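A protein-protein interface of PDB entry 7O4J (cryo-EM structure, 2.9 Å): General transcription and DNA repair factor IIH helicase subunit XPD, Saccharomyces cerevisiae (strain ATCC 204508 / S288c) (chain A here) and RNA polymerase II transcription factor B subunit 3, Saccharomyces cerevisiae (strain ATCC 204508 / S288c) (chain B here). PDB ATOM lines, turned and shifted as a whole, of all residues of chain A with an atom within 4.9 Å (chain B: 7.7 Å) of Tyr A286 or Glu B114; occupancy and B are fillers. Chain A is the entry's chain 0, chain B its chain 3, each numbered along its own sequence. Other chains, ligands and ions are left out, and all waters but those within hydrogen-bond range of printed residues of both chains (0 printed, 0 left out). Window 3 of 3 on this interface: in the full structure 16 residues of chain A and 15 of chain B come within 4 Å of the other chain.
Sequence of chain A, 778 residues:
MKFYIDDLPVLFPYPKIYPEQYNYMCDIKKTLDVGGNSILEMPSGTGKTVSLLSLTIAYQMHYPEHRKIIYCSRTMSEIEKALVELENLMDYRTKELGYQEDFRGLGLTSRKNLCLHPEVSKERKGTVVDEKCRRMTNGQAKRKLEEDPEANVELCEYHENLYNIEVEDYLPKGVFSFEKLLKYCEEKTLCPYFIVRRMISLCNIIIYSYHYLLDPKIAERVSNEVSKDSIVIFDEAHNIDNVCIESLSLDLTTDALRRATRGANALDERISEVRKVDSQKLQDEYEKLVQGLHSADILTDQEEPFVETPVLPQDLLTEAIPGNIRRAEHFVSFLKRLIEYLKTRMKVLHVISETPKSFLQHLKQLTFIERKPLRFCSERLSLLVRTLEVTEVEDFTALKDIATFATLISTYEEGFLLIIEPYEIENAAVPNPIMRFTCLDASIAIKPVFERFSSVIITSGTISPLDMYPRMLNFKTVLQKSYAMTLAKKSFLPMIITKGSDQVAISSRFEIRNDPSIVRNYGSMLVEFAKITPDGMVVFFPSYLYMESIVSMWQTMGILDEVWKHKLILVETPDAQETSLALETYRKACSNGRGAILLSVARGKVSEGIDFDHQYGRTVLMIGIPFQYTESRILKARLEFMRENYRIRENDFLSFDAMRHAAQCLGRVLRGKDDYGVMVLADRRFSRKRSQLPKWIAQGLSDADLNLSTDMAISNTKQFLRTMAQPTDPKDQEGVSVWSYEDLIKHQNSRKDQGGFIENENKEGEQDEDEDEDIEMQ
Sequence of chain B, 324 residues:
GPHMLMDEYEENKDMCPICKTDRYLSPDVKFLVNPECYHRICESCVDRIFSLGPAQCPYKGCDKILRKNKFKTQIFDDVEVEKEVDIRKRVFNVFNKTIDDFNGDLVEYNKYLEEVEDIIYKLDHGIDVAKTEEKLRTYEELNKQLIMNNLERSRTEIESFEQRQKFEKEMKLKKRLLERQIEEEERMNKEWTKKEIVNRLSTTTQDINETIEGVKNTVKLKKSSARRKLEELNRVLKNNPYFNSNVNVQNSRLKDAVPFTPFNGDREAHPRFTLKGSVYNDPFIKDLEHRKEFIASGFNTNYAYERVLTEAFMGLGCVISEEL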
ATOM      1  N   LEU A 282      21.898   9.043  15.623  1.00  0.00           N
ATOM      2  CA  LEU A 282      21.367   9.685  16.819  1.00  0.00           C
ATOM      3  C   LEU A 282      22.294   9.478  18.010  1.00  0.00           C
ATOM      4  O   LEU A 282      22.583  10.416  18.761  1.00  0.00           O
ATOM      5  CB  LEU A 282      19.970   9.140  17.126  1.00  0.00           C
ATOM      6  CG  LEU A 282      18.795   9.837  16.435  1.00  0.00           C
ATOM      7  CD1 LEU A 282      18.654  11.273  16.916  1.00  0.00           C
ATOM      8  CD2 LEU A 282      18.956   9.789  14.924  1.00  0.00           C
ATOM      9  N   GLN A 283      22.775   8.247  18.196  1.00  0.00           N
ATOM     10  CA  GLN A 283      23.671   7.969  19.314  1.00  0.00           C
ATOM     11  C   GLN A 283      24.984   8.727  19.170  1.00  0.00           C
ATOM     12  O   GLN A 283      25.522   9.241  20.157  1.00  0.00           O
ATOM     13  CB  GLN A 283      23.926   6.466  19.419  1.00  0.00           C
ATOM     14  CG  GLN A 283      24.574   6.037  20.729  1.00  0.00           C
ATOM     15  CD  GLN A 283      23.710   6.337  21.939  1.00  0.00           C
ATOM     16  OE1 GLN A 283      24.175   6.928  22.915  1.00  0.00           O
ATOM     17  NE2 GLN A 283      22.448   5.930  21.883  1.00  0.00           N
ATOM     18  N   ASP A 284      25.518   8.804  17.949  1.00  0.00           N
ATOM     19  CA  ASP A 284      26.770   9.523  17.741  1.00  0.00           C
ATOM     20  C   ASP A 284      26.632  10.989  18.129  1.00  0.00           C
ATOM     21  O   ASP A 284      27.506  11.546  18.804  1.00  0.00           O
ATOM     22  CB  ASP A 284      27.212   9.393  16.283  1.00  0.00           C
ATOM     23  CG  ASP A 284      28.721   9.379  16.127  1.00  0.00           C
ATOM     24  OD1 ASP A 284      29.404   8.755  16.966  1.00  0.00           O
ATOM     25  OD2 ASP A 284      29.224   9.993  15.164  1.00  0.00           O
ATOM     26  N   GLU A 285      25.539  11.631  17.715  1.00  0.00           N
ATOM     27  CA  GLU A 285      25.306  13.015  18.111  1.00  0.00           C
ATOM     28  C   GLU A 285      25.120  13.128  19.618  1.00  0.00           C
ATOM     29  O   GLU A 285      25.666  14.038  20.251  1.00  0.00           O
ATOM     30  CB  GLU A 285      24.085  13.570  17.377  1.00  0.00           C
ATOM     31  CG  GLU A 285      23.796  15.042  17.653  1.00  0.00           C
ATOM     32  CD  GLU A 285      22.321  15.377  17.547  1.00  0.00           C
ATOM     33  OE1 GLU A 285      21.956  16.189  16.672  1.00  0.00           O
ATOM     34  OE2 GLU A 285      21.528  14.828  18.340  1.00  0.00           O
ATOM     35  N   TYR A 286      24.358  12.206  20.211  1.00  0.00           N
ATOM     36  CA  TYR A 286      24.124  12.259  21.650  1.00  0.00           C
ATOM     37  C   TYR A 286      25.428  12.128  22.424  1.00  0.00           C
ATOM     38  O   TYR A 286      25.643  12.830  23.419  1.00  0.00           O
ATOM     39  CB  TYR A 286      23.144  11.159  22.060  1.00  0.00           C
ATOM     40  CG  TYR A 286      23.029  10.968  23.556  1.00  0.00           C
ATOM     41  CD1 TYR A 286      22.182  11.766  24.315  1.00  0.00           C
ATOM     42  CD2 TYR A 286      23.766   9.991  24.208  1.00  0.00           C
ATOM     43  CE1 TYR A 286      22.075  11.593  25.682  1.00  0.00           C
ATOM     44  CE2 TYR A 286      23.666   9.812  25.572  1.00  0.00           C
ATOM     45  CZ  TYR A 286      22.821  10.616  26.305  1.00  0.00           C
ATOM     46  OH  TYR A 286      22.722  10.433  27.664  1.00  0.00           O
ATOM     47  N   GLU A 287      26.315  11.232  21.983  1.00  0.00           N
ATOM     48  CA  GLU A 287      27.585  11.048  22.675  1.00  0.00           C
ATOM     49  C   GLU A 287      28.382  12.346  22.711  1.00  0.00           C
ATOM     50  O   GLU A 287      28.874  12.758  23.767  1.00  0.00           O
ATOM     51  CB  GLU A 287      28.392   9.940  21.996  1.00  0.00           C
ATOM     52  CG  GLU A 287      29.692   9.568  22.705  1.00  0.00           C
ATOM     53  CD  GLU A 287      29.542   9.461  24.210  1.00  0.00           C
ATOM     54  OE1 GLU A 287      30.450   9.922  24.933  1.00  0.00           O
ATOM     55  OE2 GLU A 287      28.519   8.911  24.671  1.00  0.00           O
ATOM     56  N   LYS A 288      28.513  13.013  21.561  1.00  0.00           N
ATOM     57  CA  LYS A 288      29.261  14.264  21.521  1.00  0.00           C
ATOM     58  C   LYS A 288      28.580  15.347  22.345  1.00  0.00           C
ATOM     59  O   LYS A 288      29.260  16.165  22.977  1.00  0.00           O
ATOM     60  CB  LYS A 288      29.437  14.723  20.074  1.00  0.00           C
ATOM     61  CG  LYS A 288      30.394  13.850  19.270  1.00  0.00           C
ATOM     62  CD  LYS A 288      29.909  13.605  17.848  1.00  0.00           C
ATOM     63  CE  LYS A 288      30.465  14.641  16.885  1.00  0.00           C
ATOM     64  NZ  LYS A 288      30.116  14.336  15.471  1.00  0.00           N
ATOM     65  N   LEU A 289      27.246  15.375  22.354  1.00  0.00           N
ATOM     66  CA  LEU A 289      26.537  16.361  23.161  1.00  0.00           C
ATOM     67  C   LEU A 289      26.831  16.171  24.644  1.00  0.00           C
ATOM     68  O   LEU A 289      27.020  17.149  25.375  1.00  0.00           O
ATOM     69  CB  LEU A 289      25.033  16.270  22.896  1.00  0.00           C
ATOM     70  CG  LEU A 289      24.540  16.812  21.551  1.00  0.00           C
ATOM     71  CD1 LEU A 289      23.026  16.706  21.457  1.00  0.00           C
ATOM     72  CD2 LEU A 289      24.985  18.251  21.344  1.00  0.00           C
ATOM     73  N   VAL A 290      26.872  14.920  25.104  1.00  0.00           N
ATOM     74  CA  VAL A 290      27.190  14.653  26.504  1.00  0.00           C
ATOM     75  C   VAL A 290      28.594  15.142  26.835  1.00  0.00           C
ATOM     76  O   VAL A 290      28.839  15.681  27.920  1.00  0.00           O
ATOM     77  CB  VAL A 290      27.032  13.154  26.815  1.00  0.00           C
ATOM     78  CG1 VAL A 290      27.446  12.866  28.247  1.00  0.00           C
ATOM     79  CG2 VAL A 290      25.597  12.705  26.584  1.00  0.00           C
ATOM     80  N   GLY A 323      20.709  19.128  29.002  1.00  0.00           N
ATOM     81  CA  GLY A 323      20.283  17.766  29.210  1.00  0.00           C
ATOM     82  C   GLY A 323      18.813  17.528  28.924  1.00  0.00           C
ATOM     83  O   GLY A 323      18.444  16.426  28.504  1.00  0.00           O
ATOM     84  N   ARG A 326      18.711  17.184  25.214  1.00  0.00           N
ATOM     85  CA  ARG A 326      19.859  16.423  24.740  1.00  0.00           C
ATOM     86  C   ARG A 326      19.477  15.334  23.747  1.00  0.00           C
ATOM     87  O   ARG A 326      20.283  15.009  22.868  1.00  0.00           O
ATOM     88  CB  ARG A 326      20.591  15.802  25.929  1.00  0.00           C
ATOM     89  CG  ARG A 326      21.990  15.318  25.615  1.00  0.00           C
ATOM     90  CD  ARG A 326      22.737  14.967  26.887  1.00  0.00           C
ATOM     91  NE  ARG A 326      23.359  16.139  27.494  1.00  0.00           N
ATOM     92  CZ  ARG A 326      24.082  16.112  28.610  1.00  0.00           C
ATOM     93  NH1 ARG A 326      24.279  14.969  29.253  1.00  0.00           N
ATOM     94  NH2 ARG A 326      24.609  17.232  29.084  1.00  0.00           N
ATOM     95  N   ARG A 327      18.281  14.766  23.862  1.00  0.00           N
ATOM     96  CA  ARG A 327      17.812  13.726  22.962  1.00  0.00           C
ATOM     97  C   ARG A 327      16.855  14.317  21.936  1.00  0.00           C
ATOM     98  O   ARG A 327      16.243  15.366  22.153  1.00  0.00           O
ATOM     99  CB  ARG A 327      17.124  12.598  23.737  1.00  0.00           C
ATOM    100  CG  ARG A 327      18.088  11.695  24.492  1.00  0.00           C
ATOM    101  CD  ARG A 327      18.765  10.699  23.563  1.00  0.00           C
ATOM    102  NE  ARG A 327      19.357   9.581  24.292  1.00  0.00           N
ATOM    103  CZ  ARG A 327      19.757   8.444  23.727  1.00  0.00           C
ATOM    104  NH1 ARG A 327      19.632   8.265  22.419  1.00  0.00           N
ATOM    105  NH2 ARG A 327      20.285   7.484  24.474  1.00  0.00           N
ATOM    106  N   HIS A 330      13.013  14.364  23.069  1.00  0.00           N
ATOM    107  CA  HIS A 330      12.796  15.311  24.158  1.00  0.00           C
ATOM    108  C   HIS A 330      12.863  16.748  23.658  1.00  0.00           C
ATOM    109  O   HIS A 330      12.059  17.594  24.065  1.00  0.00           O
ATOM    110  CB  HIS A 330      13.818  15.078  25.269  1.00  0.00           C
ATOM    111  CG  HIS A 330      13.805  13.684  25.814  1.00  0.00           C
ATOM    112  ND1 HIS A 330      14.920  13.088  26.363  1.00  0.00           N
ATOM    113  CD2 HIS A 330      12.813  12.766  25.890  1.00  0.00           C
ATOM    114  CE1 HIS A 330      14.614  11.865  26.756  1.00  0.00           C
ATOM    115  NE2 HIS A 330      13.341  11.645  26.481  1.00  0.00           N
ATOM    116  N   GLU B 108      26.178  15.719  36.890  1.00  0.00           N
ATOM    117  CA  GLU B 108      25.138  15.010  37.628  1.00  0.00           C
ATOM    118  C   GLU B 108      23.774  15.649  37.403  1.00  0.00           C
ATOM    119  O   GLU B 108      22.770  14.947  37.237  1.00  0.00           O
ATOM    120  CB  GLU B 108      25.478  14.984  39.119  1.00  0.00           C
ATOM    121  CG  GLU B 108      26.720  14.173  39.465  1.00  0.00           C
ATOM    122  CD  GLU B 108      26.663  12.751  38.939  1.00  0.00           C
ATOM    123  OE1 GLU B 108      27.428  12.432  38.005  1.00  0.00           O
ATOM    124  OE2 GLU B 108      25.854  11.954  39.459  1.00  0.00           O
ATOM    125  N   TYR B 109      23.718  16.982  37.396  1.00  0.00           N
ATOM    126  CA  TYR B 109      22.447  17.669  37.194  1.00  0.00           C
ATOM    127  C   TYR B 109      21.869  17.357  35.819  1.00  0.00           C
ATOM    128  O   TYR B 109      20.669  17.097  35.679  1.00  0.00           O
ATOM    129  CB  TYR B 109      22.638  19.176  37.370  1.00  0.00           C
ATOM    130  CG  TYR B 109      21.367  19.989  37.248  1.00  0.00           C
ATOM    131  CD1 TYR B 109      20.140  19.466  37.634  1.00  0.00           C
ATOM    132  CD2 TYR B 109      21.397  21.282  36.744  1.00  0.00           C
ATOM    133  CE1 TYR B 109      18.980  20.208  37.523  1.00  0.00           C
ATOM    134  CE2 TYR B 109      20.242  22.032  36.630  1.00  0.00           C
ATOM    135  CZ  TYR B 109      19.037  21.490  37.021  1.00  0.00           C
ATOM    136  OH  TYR B 109      17.885  22.233  36.907  1.00  0.00           O
ATOM    137  N   ASN B 110      22.716  17.379  34.786  1.00  0.00           N
ATOM    138  CA  ASN B 110      22.237  17.099  33.437  1.00  0.00           C
ATOM    139  C   ASN B 110      21.751  15.660  33.316  1.00  0.00           C
ATOM    140  O   ASN B 110      20.730  15.395  32.669  1.00  0.00           O
ATOM    141  CB  ASN B 110      23.343  17.386  32.422  1.00  0.00           C
ATOM    142  CG  ASN B 110      23.618  18.868  32.266  1.00  0.00           C
ATOM    143  OD1 ASN B 110      22.909  19.705  32.825  1.00  0.00           O
ATOM    144  ND2 ASN B 110      24.653  19.202  31.505  1.00  0.00           N
ATOM    145  N   LYS B 111      22.467  14.717  33.929  1.00  0.00           N
ATOM    146  CA  LYS B 111      22.005  13.333  33.935  1.00  0.00           C
ATOM    147  C   LYS B 111      20.676  13.208  34.667  1.00  0.00           C
ATOM    148  O   LYS B 111      19.784  12.470  34.230  1.00  0.00           O
ATOM    149  CB  LYS B 111      23.058  12.430  34.578  1.00  0.00           C
ATOM    150  CG  LYS B 111      22.966  10.972  34.152  1.00  0.00           C
ATOM    151  CD  LYS B 111      24.318  10.277  34.220  1.00  0.00           C
ATOM    152  CE  LYS B 111      24.962  10.420  35.592  1.00  0.00           C
ATOM    153  NZ  LYS B 111      24.041  10.023  36.693  1.00  0.00           N
ATOM    154  N   TYR B 112      20.526  13.922  35.782  1.00  0.00           N
ATOM    155  CA  TYR B 112      19.254  13.925  36.497  1.00  0.00           C
ATOM    156  C   TYR B 112      18.138  14.470  35.615  1.00  0.00           C
ATOM    157  O   TYR B 112      17.032  13.919  35.580  1.00  0.00           O
ATOM    158  CB  TYR B 112      19.383  14.749  37.778  1.00  0.00           C
ATOM    159  CG  TYR B 112      18.073  15.012  38.484  1.00  0.00           C
ATOM    160  CD1 TYR B 112      17.498  14.053  39.305  1.00  0.00           C
ATOM    161  CD2 TYR B 112      17.414  16.224  38.333  1.00  0.00           C
ATOM    162  CE1 TYR B 112      16.302  14.292  39.954  1.00  0.00           C
ATOM    163  CE2 TYR B 112      16.218  16.472  38.977  1.00  0.00           C
ATOM    164  CZ  TYR B 112      15.667  15.503  39.786  1.00  0.00           C
ATOM    165  OH  TYR B 112      14.475  15.746  40.430  1.00  0.00           O
ATOM    166  N   LEU B 113      18.414  15.557  34.891  1.00  0.00           N
ATOM    167  CA  LEU B 113      17.410  16.119  33.995  1.00  0.00           C
ATOM    168  C   LEU B 113      17.034  15.130  32.900  1.00  0.00           C
ATOM    169  O   LEU B 113      15.852  14.978  32.570  1.00  0.00           O
ATOM    170  CB  LEU B 113      17.927  17.421  33.382  1.00  0.00           C
ATOM    171  CG  LEU B 113      17.978  18.651  34.292  1.00  0.00           C
ATOM    172  CD1 LEU B 113      18.481  19.854  33.512  1.00  0.00           C
ATOM    173  CD2 LEU B 113      16.616  18.946  34.904  1.00  0.00           C
ATOM    174  N   GLU B 114      18.026  14.450  32.323  1.00  0.00           N
ATOM    175  CA  GLU B 114      17.737  13.481  31.271  1.00  0.00           C
ATOM    176  C   GLU B 114      16.877  12.340  31.799  1.00  0.00           C
ATOM    177  O   GLU B 114      15.955  11.880  31.116  1.00  0.00           O
ATOM    178  CB  GLU B 114      19.039  12.941  30.683  1.00  0.00           C
ATOM    179  CG  GLU B 114      18.836  11.901  29.594  1.00  0.00           C
ATOM    180  CD  GLU B 114      20.085  11.667  28.769  1.00  0.00           C
ATOM    181  OE1 GLU B 114      20.078  10.742  27.929  1.00  0.00           O
ATOM    182  OE2 GLU B 114      21.074  12.406  28.959  1.00  0.00           O
ATOM    183  N   GLU B 115      17.166  11.868  33.014  1.00  0.00           N
ATOM    184  CA  GLU B 115      16.364  10.799  33.597  1.00  0.00           C
ATOM    185  C   GLU B 115      14.914  11.233  33.767  1.00  0.00           C
ATOM    186  O   GLU B 115      13.990  10.468  33.469  1.00  0.00           O
ATOM    187  CB  GLU B 115      16.957  10.374  34.940  1.00  0.00           C
ATOM    188  CG  GLU B 115      17.824   9.129  34.868  1.00  0.00           C
ATOM    189  CD  GLU B 115      18.484   8.799  36.192  1.00  0.00           C
ATOM    190  OE1 GLU B 115      18.603   9.707  37.041  1.00  0.00           O
ATOM    191  OE2 GLU B 115      18.883   7.631  36.384  1.00  0.00           O
ATOM    192  N   VAL B 116      14.695  12.461  34.241  1.00  0.00           N
ATOM    193  CA  VAL B 116      13.333  12.952  34.421  1.00  0.00           C
ATOM    194  C   VAL B 116      12.611  13.024  33.082  1.00  0.00           C
ATOM    195  O   VAL B 116      11.437  12.652  32.975  1.00  0.00           O
ATOM    196  CB  VAL B 116      13.350  14.319  35.129  1.00  0.00           C
ATOM    197  CG1 VAL B 116      11.950  14.905  35.180  1.00  0.00           C
ATOM    198  CG2 VAL B 116      13.922  14.183  36.531  1.00  0.00           C
ATOM    199  N   GLU B 117      13.294  13.506  32.042  1.00  0.00           N
ATOM    200  CA  GLU B 117      12.682  13.550  30.717  1.00  0.00           C
ATOM    201  C   GLU B 117      12.341  12.149  30.227  1.00  0.00           C
ATOM    202  O   GLU B 117      11.276  11.933  29.638  1.00  0.00           O
ATOM    203  CB  GLU B 117      13.614  14.250  29.729  1.00  0.00           C
ATOM    204  CG  GLU B 117      13.962  15.680  30.108  1.00  0.00           C
ATOM    205  CD  GLU B 117      12.921  16.680  29.641  1.00  0.00           C
ATOM    206  OE1 GLU B 117      12.462  16.568  28.486  1.00  0.00           O
ATOM    207  OE2 GLU B 117      12.563  17.579  30.431  1.00  0.00           O
ATOM    208  N   ASP B 118      13.233  11.184  30.460  1.00  0.00           N
ATOM    209  CA  ASP B 118      12.940   9.805  30.084  1.00  0.00           C
ATOM    210  C   ASP B 118      11.714   9.290  30.827  1.00  0.00           C
ATOM    211  O   ASP B 118      10.870   8.598  30.245  1.00  0.00           O
ATOM    212  CB  ASP B 118      14.154   8.919  30.367  1.00  0.00           C
ATOM    213  CG  ASP B 118      14.006   7.520  29.796  1.00  0.00           C
ATOM    214  OD1 ASP B 118      12.921   6.919  29.945  1.00  0.00           O
ATOM    215  OD2 ASP B 118      14.981   7.018  29.198  1.00  0.00           O
ATOM    216  N   ILE B 119      11.597   9.619  32.114  1.00  0.00           N
ATOM    217  CA  ILE B 119      10.425   9.212  32.884  1.00  0.00           C
ATOM    218  C   ILE B 119       9.164   9.813  32.278  1.00  0.00           C
ATOM    219  O   ILE B 119       8.148   9.131  32.107  1.00  0.00           O
ATOM    220  CB  ILE B 119      10.591   9.620  34.360  1.00  0.00           C
ATOM    221  CG1 ILE B 119      11.674   8.759  35.020  1.00  0.00           C
ATOM    222  CG2 ILE B 119       9.261   9.503  35.098  1.00  0.00           C
ATOM    223  CD1 ILE B 119      11.881   9.039  36.496  1.00  0.00           C
ATOM    224  N   ILE B 120       9.212  11.104  31.944  1.00  0.00           N
ATOM    225  CA  ILE B 120       8.049  11.762  31.357  1.00  0.00           C
ATOM    226  C   ILE B 120       7.709  11.136  30.012  1.00  0.00           C
ATOM    227  O   ILE B 120       6.536  10.895  29.701  1.00  0.00           O
ATOM    228  CB  ILE B 120       8.302  13.275  31.231  1.00  0.00           C
ATOM    229  CG1 ILE B 120       8.352  13.911  32.622  1.00  0.00           C
ATOM    230  CG2 ILE B 120       7.223  13.924  30.369  1.00  0.00           C
ATOM    231  CD1 ILE B 120       8.739  15.373  32.624  1.00  0.00           C
ATOM    232  N   TYR B 121       8.726  10.864  29.192  1.00  0.00           N
ATOM    233  CA  TYR B 121       8.479  10.265  27.886  1.00  0.00           C
ATOM    234  C   TYR B 121       7.812   8.902  28.023  1.00  0.00           C
ATOM    235  O   TYR B 121       6.858   8.594  27.299  1.00  0.00           O
ATOM    236  CB  TYR B 121       9.792  10.143  27.113  1.00  0.00           C
ATOM    237  CG  TYR B 121       9.615   9.853  25.641  1.00  0.00           C
ATOM    238  CD1 TYR B 121       9.464  10.885  24.725  1.00  0.00           C
ATOM    239  CD2 TYR B 121       9.601   8.549  25.166  1.00  0.00           C
ATOM    240  CE1 TYR B 121       9.303  10.627  23.379  1.00  0.00           C
ATOM    241  CE2 TYR B 121       9.440   8.280  23.821  1.00  0.00           C
ATOM    242  CZ  TYR B 121       9.292   9.322  22.932  1.00  0.00           C
ATOM    243  OH  TYR B 121       9.132   9.060  21.591  1.00  0.00           O
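Tyr A286 touches one residue of chain B. Of the printed residues of chain A, Asn B110 touches Arg A326 (3.1 Å). Of the printed residues of chain A, Glu B117 touches His A330 (3.8 Å). Leu A289 touches none of the printed residues of chain B. Lys A288 touches none of the printed residues of chain B. The nearest residue of chain A that does not touch Glu B114 is Gly A323 (4.1 Å).
OE1 of Glu B114 sits at hydrogen-bond distance from OH of Tyr A286. The side-chain amide nitrogen (ND2) of Asn B110 sits close to the guanidinium group (NH2) of Arg A326 (3.1 Å). NE of Arg A327 lies within salt-bridge range of OE1 of Glu B114 (3.9 Å).
Of the 14 printed residues of chain B, 4 touch a printed residue of chain A. Printed residues of chain B that touch a printed residue of chain A: Asn B110, Glu B114, Glu B117 and Tyr B121. Along chain B the printed residues that touch a printed residue of chain A span positions 110 to 121. Among the printed residues, Asp or Glu carboxylates within 4 Å of a Lys or Arg side-chain nitrogen of the other chain: Arg A327 with Glu B114.
Arg A326 touches Glu B114 (CD to OE2, 3.7 Å). His A330 touches Glu B117 (NE2 to O, 3.8 Å). CB of Tyr B121 touches NE2 of His A330, at 3.9 Å.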
